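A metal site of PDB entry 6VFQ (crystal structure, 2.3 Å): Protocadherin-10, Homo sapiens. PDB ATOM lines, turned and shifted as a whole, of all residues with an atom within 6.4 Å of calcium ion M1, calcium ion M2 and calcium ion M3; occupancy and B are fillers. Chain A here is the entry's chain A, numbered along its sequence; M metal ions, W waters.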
ATOM      1  N   GLU A 244       2.715  -7.192   4.543  1.00  0.00           N
ATOM      2  CA  GLU A 244       1.716  -8.210   4.288  1.00  0.00           C
ATOM      3  C   GLU A 244       0.419  -7.823   4.967  1.00  0.00           C
ATOM      4  O   GLU A 244       0.390  -7.028   5.915  1.00  0.00           O
ATOM      5  CB  GLU A 244       2.200  -9.590   4.765  1.00  0.00           C
ATOM      6  CG  GLU A 244       2.143  -9.793   6.258  1.00  0.00           C
ATOM      7  CD  GLU A 244       2.483 -11.214   6.730  1.00  0.00           C
ATOM      8  OE1 GLU A 244       1.998 -12.210   6.128  1.00  0.00           O
ATOM      9  OE2 GLU A 244       3.222 -11.320   7.729  1.00  0.00           O
ATOM     10  N   ASN A 245      -0.669  -8.366   4.473  1.00  0.00           N
ATOM     11  CA  ASN A 245      -2.006  -7.993   4.939  1.00  0.00           C
ATOM     12  C   ASN A 245      -2.353  -6.521   4.653  1.00  0.00           C
ATOM     13  O   ASN A 245      -3.327  -5.997   5.215  1.00  0.00           O
ATOM     14  CB  ASN A 245      -2.158  -8.298   6.438  1.00  0.00           C
ATOM     15  CG  ASN A 245      -1.798  -9.734   6.778  1.00  0.00           C
ATOM     16  OD1 ASN A 245      -2.144 -10.661   6.033  1.00  0.00           O
ATOM     17  ND2 ASN A 245      -1.103  -9.931   7.886  1.00  0.00           N
ATOM     18  N   LEU A 299      -1.955  -9.891   0.532  1.00  0.00           N
ATOM     19  CA  LEU A 299      -0.541 -10.187   0.440  1.00  0.00           C
ATOM     20  C   LEU A 299      -0.126 -10.991   1.659  1.00  0.00           C
ATOM     21  O   LEU A 299      -0.189 -10.477   2.789  1.00  0.00           O
ATOM     22  CB  LEU A 299       0.256  -8.903   0.364  1.00  0.00           C
ATOM     23  CG  LEU A 299      -0.076  -8.046  -0.852  1.00  0.00           C
ATOM     24  CD1 LEU A 299       0.658  -6.709  -0.800  1.00  0.00           C
ATOM     25  CD2 LEU A 299       0.288  -8.789  -2.126  1.00  0.00           C
ATOM     26  N   ASP A 300       0.295 -12.232   1.450  1.00  0.00           N
ATOM     27  CA  ASP A 300       0.708 -13.127   2.531  1.00  0.00           C
ATOM     28  C   ASP A 300       2.204 -13.419   2.400  1.00  0.00           C
ATOM     29  O   ASP A 300       2.619 -14.138   1.485  1.00  0.00           O
ATOM     30  CB  ASP A 300      -0.103 -14.418   2.523  1.00  0.00           C
ATOM     31  CG  ASP A 300       0.377 -15.407   3.568  1.00  0.00           C
ATOM     32  OD1 ASP A 300       1.182 -15.032   4.463  1.00  0.00           O
ATOM     33  OD2 ASP A 300      -0.052 -16.569   3.508  1.00  0.00           O
ATOM     34  N   TYR A 301       3.001 -12.885   3.321  1.00  0.00           N
ATOM     35  CA  TYR A 301       4.439 -13.147   3.327  1.00  0.00           C
ATOM     36  C   TYR A 301       4.727 -14.649   3.381  1.00  0.00           C
ATOM     37  O   TYR A 301       5.602 -15.149   2.665  1.00  0.00           O
ATOM     38  CB  TYR A 301       5.084 -12.452   4.520  1.00  0.00           C
ATOM     39  CG  TYR A 301       6.564 -12.642   4.596  1.00  0.00           C
ATOM     40  CD1 TYR A 301       7.122 -13.724   5.260  1.00  0.00           C
ATOM     41  CD2 TYR A 301       7.411 -11.736   3.996  1.00  0.00           C
ATOM     42  CE1 TYR A 301       8.516 -13.891   5.321  1.00  0.00           C
ATOM     43  CE2 TYR A 301       8.773 -11.887   4.050  1.00  0.00           C
ATOM     44  CZ  TYR A 301       9.327 -12.959   4.698  1.00  0.00           C
ATOM     45  OH  TYR A 301      10.697 -13.063   4.719  1.00  0.00           O
ATOM     46  N   GLU A 302       4.007 -15.384   4.234  1.00  0.00           N
ATOM     47  CA  GLU A 302       4.270 -16.799   4.358  1.00  0.00           C
ATOM     48  C   GLU A 302       3.916 -17.567   3.094  1.00  0.00           C
ATOM     49  O   GLU A 302       4.229 -18.758   3.009  1.00  0.00           O
ATOM     50  CB  GLU A 302       3.524 -17.379   5.571  1.00  0.00           C
ATOM     51  CG  GLU A 302       4.134 -16.979   6.915  1.00  0.00           C
ATOM     52  CD  GLU A 302       3.851 -15.533   7.336  1.00  0.00           C
ATOM     53  OE1 GLU A 302       2.673 -15.094   7.309  1.00  0.00           O
ATOM     54  OE2 GLU A 302       4.816 -14.827   7.718  1.00  0.00           O
ATOM     55  N   GLU A 303       3.274 -16.926   2.123  1.00  0.00           N
ATOM     56  CA  GLU A 303       3.038 -17.513   0.812  1.00  0.00           C
ATOM     57  C   GLU A 303       4.132 -17.150  -0.180  1.00  0.00           C
ATOM     58  O   GLU A 303       4.614 -18.011  -0.921  1.00  0.00           O
ATOM     59  CB  GLU A 303       1.685 -17.055   0.275  1.00  0.00           C
ATOM     60  CG  GLU A 303       1.313 -17.637  -1.074  1.00  0.00           C
ATOM     61  CD  GLU A 303       0.022 -17.054  -1.608  1.00  0.00           C
ATOM     62  OE1 GLU A 303      -0.531 -16.136  -0.959  1.00  0.00           O
ATOM     63  OE2 GLU A 303      -0.443 -17.510  -2.684  1.00  0.00           O
ATOM     64  N   LEU A 332       6.557  -7.506   3.273  1.00  0.00           N
ATOM     65  CA  LEU A 332       7.205  -7.419   4.574  1.00  0.00           C
ATOM     66  C   LEU A 332       6.435  -8.270   5.570  1.00  0.00           C
ATOM     67  O   LEU A 332       5.203  -8.204   5.627  1.00  0.00           O
ATOM     68  CB  LEU A 332       7.276  -5.974   5.050  1.00  0.00           C
ATOM     69  CG  LEU A 332       8.010  -5.026   4.120  1.00  0.00           C
ATOM     70  CD1 LEU A 332       7.907  -3.619   4.669  1.00  0.00           C
ATOM     71  CD2 LEU A 332       9.464  -5.434   3.987  1.00  0.00           C
ATOM     72  N   ASP A 333       7.158  -9.089   6.322  1.00  0.00           N
ATOM     73  CA  ASP A 333       6.535 -10.018   7.250  1.00  0.00           C
ATOM     74  C   ASP A 333       5.950  -9.261   8.438  1.00  0.00           C
ATOM     75  O   ASP A 333       6.591  -8.377   8.998  1.00  0.00           O
ATOM     76  CB  ASP A 333       7.577 -11.053   7.696  1.00  0.00           C
ATOM     77  CG  ASP A 333       7.108 -11.950   8.860  1.00  0.00           C
ATOM     78  OD1 ASP A 333       6.080 -12.683   8.759  1.00  0.00           O
ATOM     79  OD2 ASP A 333       7.830 -11.928   9.880  1.00  0.00           O
ATOM     80  N   ALA A 334       4.711  -9.600   8.786  1.00  0.00           N
ATOM     81  CA  ALA A 334       4.069  -9.183  10.019  1.00  0.00           C
ATOM     82  C   ALA A 334       3.930 -10.376  10.981  1.00  0.00           C
ATOM     83  O   ALA A 334       4.129 -11.530  10.611  1.00  0.00           O
ATOM     84  CB  ALA A 334       2.682  -8.596   9.723  1.00  0.00           C
ATOM     85  N   ASN A 335       3.532 -10.085  12.228  1.00  0.00           N
ATOM     86  CA  ASN A 335       3.340 -11.140  13.225  1.00  0.00           C
ATOM     87  C   ASN A 335       1.878 -11.544  13.226  1.00  0.00           C
ATOM     88  O   ASN A 335       1.081 -11.150  14.075  1.00  0.00           O
ATOM     89  CB  ASN A 335       3.806 -10.691  14.605  1.00  0.00           C
ATOM     90  CG  ASN A 335       3.880 -11.873  15.611  1.00  0.00           C
ATOM     91  OD1 ASN A 335       4.006 -13.031  15.231  1.00  0.00           O
ATOM     92  ND2 ASN A 335       3.778 -11.559  16.902  1.00  0.00           N
ATOM     93  N   ASP A 336       1.531 -12.389  12.258  1.00  0.00           N
ATOM     94  CA  ASP A 336       0.169 -12.881  12.114  1.00  0.00           C
ATOM     95  C   ASP A 336       0.044 -14.383  12.329  1.00  0.00           C
ATOM     96  O   ASP A 336      -1.016 -14.946  12.018  1.00  0.00           O
ATOM     97  CB  ASP A 336      -0.389 -12.481  10.743  1.00  0.00           C
ATOM     98  CG  ASP A 336       0.508 -12.883   9.559  1.00  0.00           C
ATOM     99  OD1 ASP A 336       1.692 -13.264   9.762  1.00  0.00           O
ATOM    100  OD2 ASP A 336       0.003 -12.814   8.416  1.00  0.00           O
ATOM    101  N   ASN A 337       1.057 -15.060  12.854  1.00  0.00           N
ATOM    102  CA  ASN A 337       0.908 -16.450  13.272  1.00  0.00           C
ATOM    103  C   ASN A 337       1.310 -16.612  14.738  1.00  0.00           C
ATOM    104  O   ASN A 337       2.370 -16.138  15.162  1.00  0.00           O
ATOM    105  CB  ASN A 337       1.731 -17.384  12.390  1.00  0.00           C
ATOM    106  CG  ASN A 337       1.208 -17.427  10.969  1.00  0.00           C
ATOM    107  OD1 ASN A 337       0.312 -18.198  10.639  1.00  0.00           O
ATOM    108  ND2 ASN A 337       1.771 -16.601  10.110  1.00  0.00           N
ATOM    109  N   ALA A 338       0.510 -17.265  15.455  1.00  0.00           N
ATOM    110  CA  ALA A 338       0.840 -17.535  16.836  1.00  0.00           C
ATOM    111  C   ALA A 338       1.649 -18.825  16.953  1.00  0.00           C
ATOM    112  O   ALA A 338       1.512 -19.720  16.111  1.00  0.00           O
ATOM    113  CB  ALA A 338      -0.428 -17.648  17.672  1.00  0.00           C
ATOM    114  N   PRO A 339       2.491 -18.931  17.977  1.00  0.00           N
ATOM    115  CA  PRO A 339       3.232 -20.188  18.212  1.00  0.00           C
ATOM    116  C   PRO A 339       2.328 -21.411  18.288  1.00  0.00           C
ATOM    117  O   PRO A 339       1.181 -21.336  18.736  1.00  0.00           O
ATOM    118  CB  PRO A 339       3.908 -19.927  19.564  1.00  0.00           C
ATOM    119  CG  PRO A 339       4.036 -18.449  19.655  1.00  0.00           C
ATOM    120  CD  PRO A 339       2.879 -17.873  18.910  1.00  0.00           C
ATOM    121  N   ASP A 367       6.559 -21.549  14.976  1.00  0.00           N
ATOM    122  CA  ASP A 367       5.901 -20.287  14.631  1.00  0.00           C
ATOM    123  C   ASP A 367       6.138 -20.005  13.147  1.00  0.00           C
ATOM    124  O   ASP A 367       7.292 -19.888  12.719  1.00  0.00           O
ATOM    125  CB  ASP A 367       6.453 -19.138  15.512  1.00  0.00           C
ATOM    126  CG  ASP A 367       5.623 -17.846  15.401  1.00  0.00           C
ATOM    127  OD1 ASP A 367       5.382 -17.361  14.273  1.00  0.00           O
ATOM    128  OD2 ASP A 367       5.221 -17.306  16.454  1.00  0.00           O
ATOM    129  N   ARG A 368       5.062 -19.916  12.365  1.00  0.00           N
ATOM    130  CA  ARG A 368       5.197 -19.795  10.913  1.00  0.00           C
ATOM    131  C   ARG A 368       5.839 -18.487  10.469  1.00  0.00           C
ATOM    132  O   ARG A 368       6.187 -18.355   9.287  1.00  0.00           O
ATOM    133  CB  ARG A 368       3.837 -19.916  10.208  1.00  0.00           C
ATOM    134  CG  ARG A 368       3.062 -21.219  10.481  1.00  0.00           C
ATOM    135  CD  ARG A 368       2.400 -21.821   9.230  1.00  0.00           C
ATOM    136  NE  ARG A 368       1.597 -20.846   8.494  1.00  0.00           N
ATOM    137  CZ  ARG A 368       1.763 -20.509   7.213  1.00  0.00           C
ATOM    138  NH1 ARG A 368       2.714 -21.077   6.475  1.00  0.00           N
ATOM    139  NH2 ARG A 368       0.961 -19.601   6.663  1.00  0.00           N
ATOM    140  N   ASP A 369       5.999 -17.531  11.378  1.00  0.00           N
ATOM    141  CA  ASP A 369       6.576 -16.242  11.044  1.00  0.00           C
ATOM    142  C   ASP A 369       8.107 -16.351  10.992  1.00  0.00           C
ATOM    143  O   ASP A 369       8.690 -17.418  11.185  1.00  0.00           O
ATOM    144  CB  ASP A 369       6.107 -15.187  12.042  1.00  0.00           C
ATOM    145  CG  ASP A 369       4.611 -14.924  11.954  1.00  0.00           C
ATOM    146  OD1 ASP A 369       4.095 -14.804  10.808  1.00  0.00           O
ATOM    147  OD2 ASP A 369       3.935 -14.854  13.009  1.00  0.00           O
ATOM    148  N   SER A 370       8.768 -15.223  10.744  1.00  0.00           N
ATOM    149  CA  SER A 370      10.215 -15.170  10.535  1.00  0.00           C
ATOM    150  C   SER A 370      10.816 -14.126  11.472  1.00  0.00           C
ATOM    151  O   SER A 370      10.130 -13.233  11.957  1.00  0.00           O
ATOM    152  CB  SER A 370      10.559 -14.823   9.079  1.00  0.00           C
ATOM    153  OG  SER A 370       9.961 -15.729   8.164  1.00  0.00           O
ATOM    154  N   GLU A 372      12.162 -12.146  14.641  1.00  0.00           N
ATOM    155  CA  GLU A 372      11.494 -11.973  15.922  1.00  0.00           C
ATOM    156  C   GLU A 372      10.066 -12.478  15.903  1.00  0.00           C
ATOM    157  O   GLU A 372       9.570 -12.999  16.908  1.00  0.00           O
ATOM    158  CB  GLU A 372      11.500 -10.498  16.323  1.00  0.00           C
ATOM    159  CG  GLU A 372      12.869  -9.912  16.652  1.00  0.00           C
ATOM    160  CD  GLU A 372      12.813  -8.407  16.846  1.00  0.00           C
ATOM    161  OE1 GLU A 372      11.807  -7.782  16.431  1.00  0.00           O
ATOM    162  OE2 GLU A 372      13.773  -7.834  17.423  1.00  0.00           O
ATOM    163  N   ASN A 373       9.349 -12.279  14.801  1.00  0.00           N
ATOM    164  CA  ASN A 373       7.956 -12.705  14.786  1.00  0.00           C
ATOM    165  C   ASN A 373       7.834 -14.218  14.923  1.00  0.00           C
ATOM    166  O   ASN A 373       6.748 -14.708  15.266  1.00  0.00           O
ATOM    167  CB  ASN A 373       7.256 -12.241  13.508  1.00  0.00           C
ATOM    168  CG  ASN A 373       7.323 -10.731  13.322  1.00  0.00           C
ATOM    169  OD1 ASN A 373       7.080  -9.958  14.256  1.00  0.00           O
ATOM    170  ND2 ASN A 373       7.652 -10.309  12.104  1.00  0.00           N
ATOM    171  N   GLY A 374       8.908 -14.960  14.648  1.00  0.00           N
ATOM    172  CA  GLY A 374       8.921 -16.404  14.749  1.00  0.00           C
ATOM    173  C   GLY A 374       9.766 -16.941  15.881  1.00  0.00           C
ATOM    174  O   GLY A 374       9.955 -18.155  15.964  1.00  0.00           O
ATOM    175  N   GLN A 375      10.290 -16.082  16.760  1.00  0.00           N
ATOM    176  CA  GLN A 375      11.067 -16.478  17.921  1.00  0.00           C
ATOM    177  C   GLN A 375      10.133 -16.685  19.102  1.00  0.00           C
ATOM    178  O   GLN A 375       9.339 -15.799  19.427  1.00  0.00           O
ATOM    179  CB  GLN A 375      12.092 -15.401  18.276  1.00  0.00           C
ATOM    180  CG  GLN A 375      13.360 -15.445  17.488  1.00  0.00           C
ATOM    181  CD  GLN A 375      14.265 -14.274  17.855  1.00  0.00           C
ATOM    182  OE1 GLN A 375      13.831 -13.325  18.520  1.00  0.00           O
ATOM    183  NE2 GLN A 375      15.521 -14.338  17.427  1.00  0.00           N
ATOM    184  N   ASP A 420       5.623 -15.546  21.142  1.00  0.00           N
ATOM    185  CA  ASP A 420       6.621 -15.035  20.214  1.00  0.00           C
ATOM    186  C   ASP A 420       6.997 -13.601  20.604  1.00  0.00           C
ATOM    187  O   ASP A 420       6.408 -13.002  21.495  1.00  0.00           O
ATOM    188  CB  ASP A 420       6.148 -15.100  18.745  1.00  0.00           C
ATOM    189  CG  ASP A 420       4.949 -14.219  18.454  1.00  0.00           C
ATOM    190  OD1 ASP A 420       4.872 -13.097  18.980  1.00  0.00           O
ATOM    191  OD2 ASP A 420       4.074 -14.656  17.680  1.00  0.00           O
ATOM    192  N   ARG A 421       7.951 -13.040  19.868  1.00  0.00           N
ATOM    193  CA  ARG A 421       8.560 -11.751  20.180  1.00  0.00           C
ATOM    194  C   ARG A 421       8.260 -10.689  19.128  1.00  0.00           C
ATOM    195  O   ARG A 421       9.095  -9.821  18.864  1.00  0.00           O
ATOM    196  CB  ARG A 421      10.068 -11.924  20.356  1.00  0.00           C
ATOM    197  CG  ARG A 421      10.422 -12.636  21.667  1.00  0.00           C
ATOM    198  CD  ARG A 421      11.900 -12.579  21.939  1.00  0.00           C
ATOM    199  NE  ARG A 421      12.397 -11.219  22.140  1.00  0.00           N
ATOM    200  CZ  ARG A 421      12.366 -10.567  23.299  1.00  0.00           C
ATOM    201  NH1 ARG A 421      11.842 -11.125  24.382  1.00  0.00           N
ATOM    202  NH2 ARG A 421      12.869  -9.336  23.374  1.00  0.00           N
ATOM    203  N   GLY A 422       7.071 -10.751  18.529  1.00  0.00           N
ATOM    204  CA  GLY A 422       6.594  -9.698  17.651  1.00  0.00           C
ATOM    205  C   GLY A 422       5.879  -8.579  18.397  1.00  0.00           C
ATOM    206  O   GLY A 422       5.752  -8.598  19.623  1.00  0.00           O
ATOM    207  N   LEU A 426       2.125 -12.585  20.227  1.00  0.00           N
ATOM    208  CA  LEU A 426       1.097 -13.604  20.192  1.00  0.00           C
ATOM    209  C   LEU A 426       1.558 -14.774  21.026  1.00  0.00           C
ATOM    210  O   LEU A 426       2.747 -15.059  21.120  1.00  0.00           O
ATOM    211  CB  LEU A 426       0.821 -14.052  18.759  1.00  0.00           C
ATOM    212  CG  LEU A 426       0.230 -12.921  17.918  1.00  0.00           C
ATOM    213  CD1 LEU A 426       0.186 -13.339  16.477  1.00  0.00           C
ATOM    214  CD2 LEU A 426      -1.156 -12.567  18.430  1.00  0.00           C
HETATM  215 CA    CA M   1       4.463 -15.282  15.308  1.00  0.00          CA
HETATM  216 CA    CA M   2       3.801 -13.240   8.976  1.00  0.00          CA
HETATM  217 CA    CA M   3       0.689 -14.183   6.672  1.00  0.00          CA
HETATM  218  O   HOH W   1      -0.293 -16.242   7.425  1.00  0.00           O
HETATM  219  O   HOH W   2      -1.328 -13.253   5.412  1.00  0.00           O
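Calcium ion M2 is bound by OD1 of Asp 336 (2.3 Å), OE2 of Glu 302 (2.3 Å), OD1 of Asp 333 (2.4 Å), OE2 of Glu 244 (2.4 Å), O of Ala 334 (2.4 Å), OD1 of Asp 369 (2.4 Å) and OE1 of Glu 302 (2.7 Å). Calcium ion M2 has seven donor atoms within binding distance.
Six residues have an atom within 4 Å of calcium ion M1: Asn 335, Asn 337, Asp 367, Asp 369, Asn 373 and Asp 420.
Calcium ion M3 is bound by OE1 of Glu 302, OD2 of Asp 336, water W1, OD1 of Asp 300, OE1 of Glu 244 and water W2. Calcium ion M3 has six donor atoms within binding distance.
Of the 27 residues printed, 4 come within 4 Å of calcium ion M3. The nearest printed residue that does not touch calcium ion M3 is Tyr 301 (4.3 Å).
The side-chain amide nitrogen (ND2) of Asn 373 is in hydrogen-bond range of the side-chain carboxylate (OD2) of Asp 333 (2.8 Å). The side-chain carboxylate of Glu 302 sits close to the side-chain amide nitrogen of Asn 337, 3.3 Å away. The side-chain amide nitrogen of Asn 337 sits close to the side-chain carboxylate of Asp 336 (3.4 Å). The backbone NH (N) of Asp 420 sits at hydrogen-bond distance from the backbone carbonyl oxygen (O) of Leu 426, 2.9 Å away. OD2 of Asp 336 sits close to ND2 of Asn 245 (3.1 Å). The side-chain carboxylate of Glu 244 sits close to the backbone NH of Tyr 301 (3.1 Å). The backbone carbonyl oxygen (O) of Leu 332 is in hydrogen-bond range of the backbone NH (N) of Glu 244, at 2.9 Å. OD1 of Asp 420 is in hydrogen-bond range of N of Gly 422, 3.2 Å away.
Calcium ion M1 is bound by O of Asn 337 (2.3 Å), OD1 of Asn 335 (2.3 Å), O of Asn 373 (2.4 Å), OD2 of Asp 369 (2.4 Å), OD2 of Asp 367 (2.4 Å), OD2 of Asp 420 (2.5 Å) and OD1 of Asp 367 (2.5 Å).
Of the 27 residues printed, 6 come within 4 Å of calcium ion M2.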
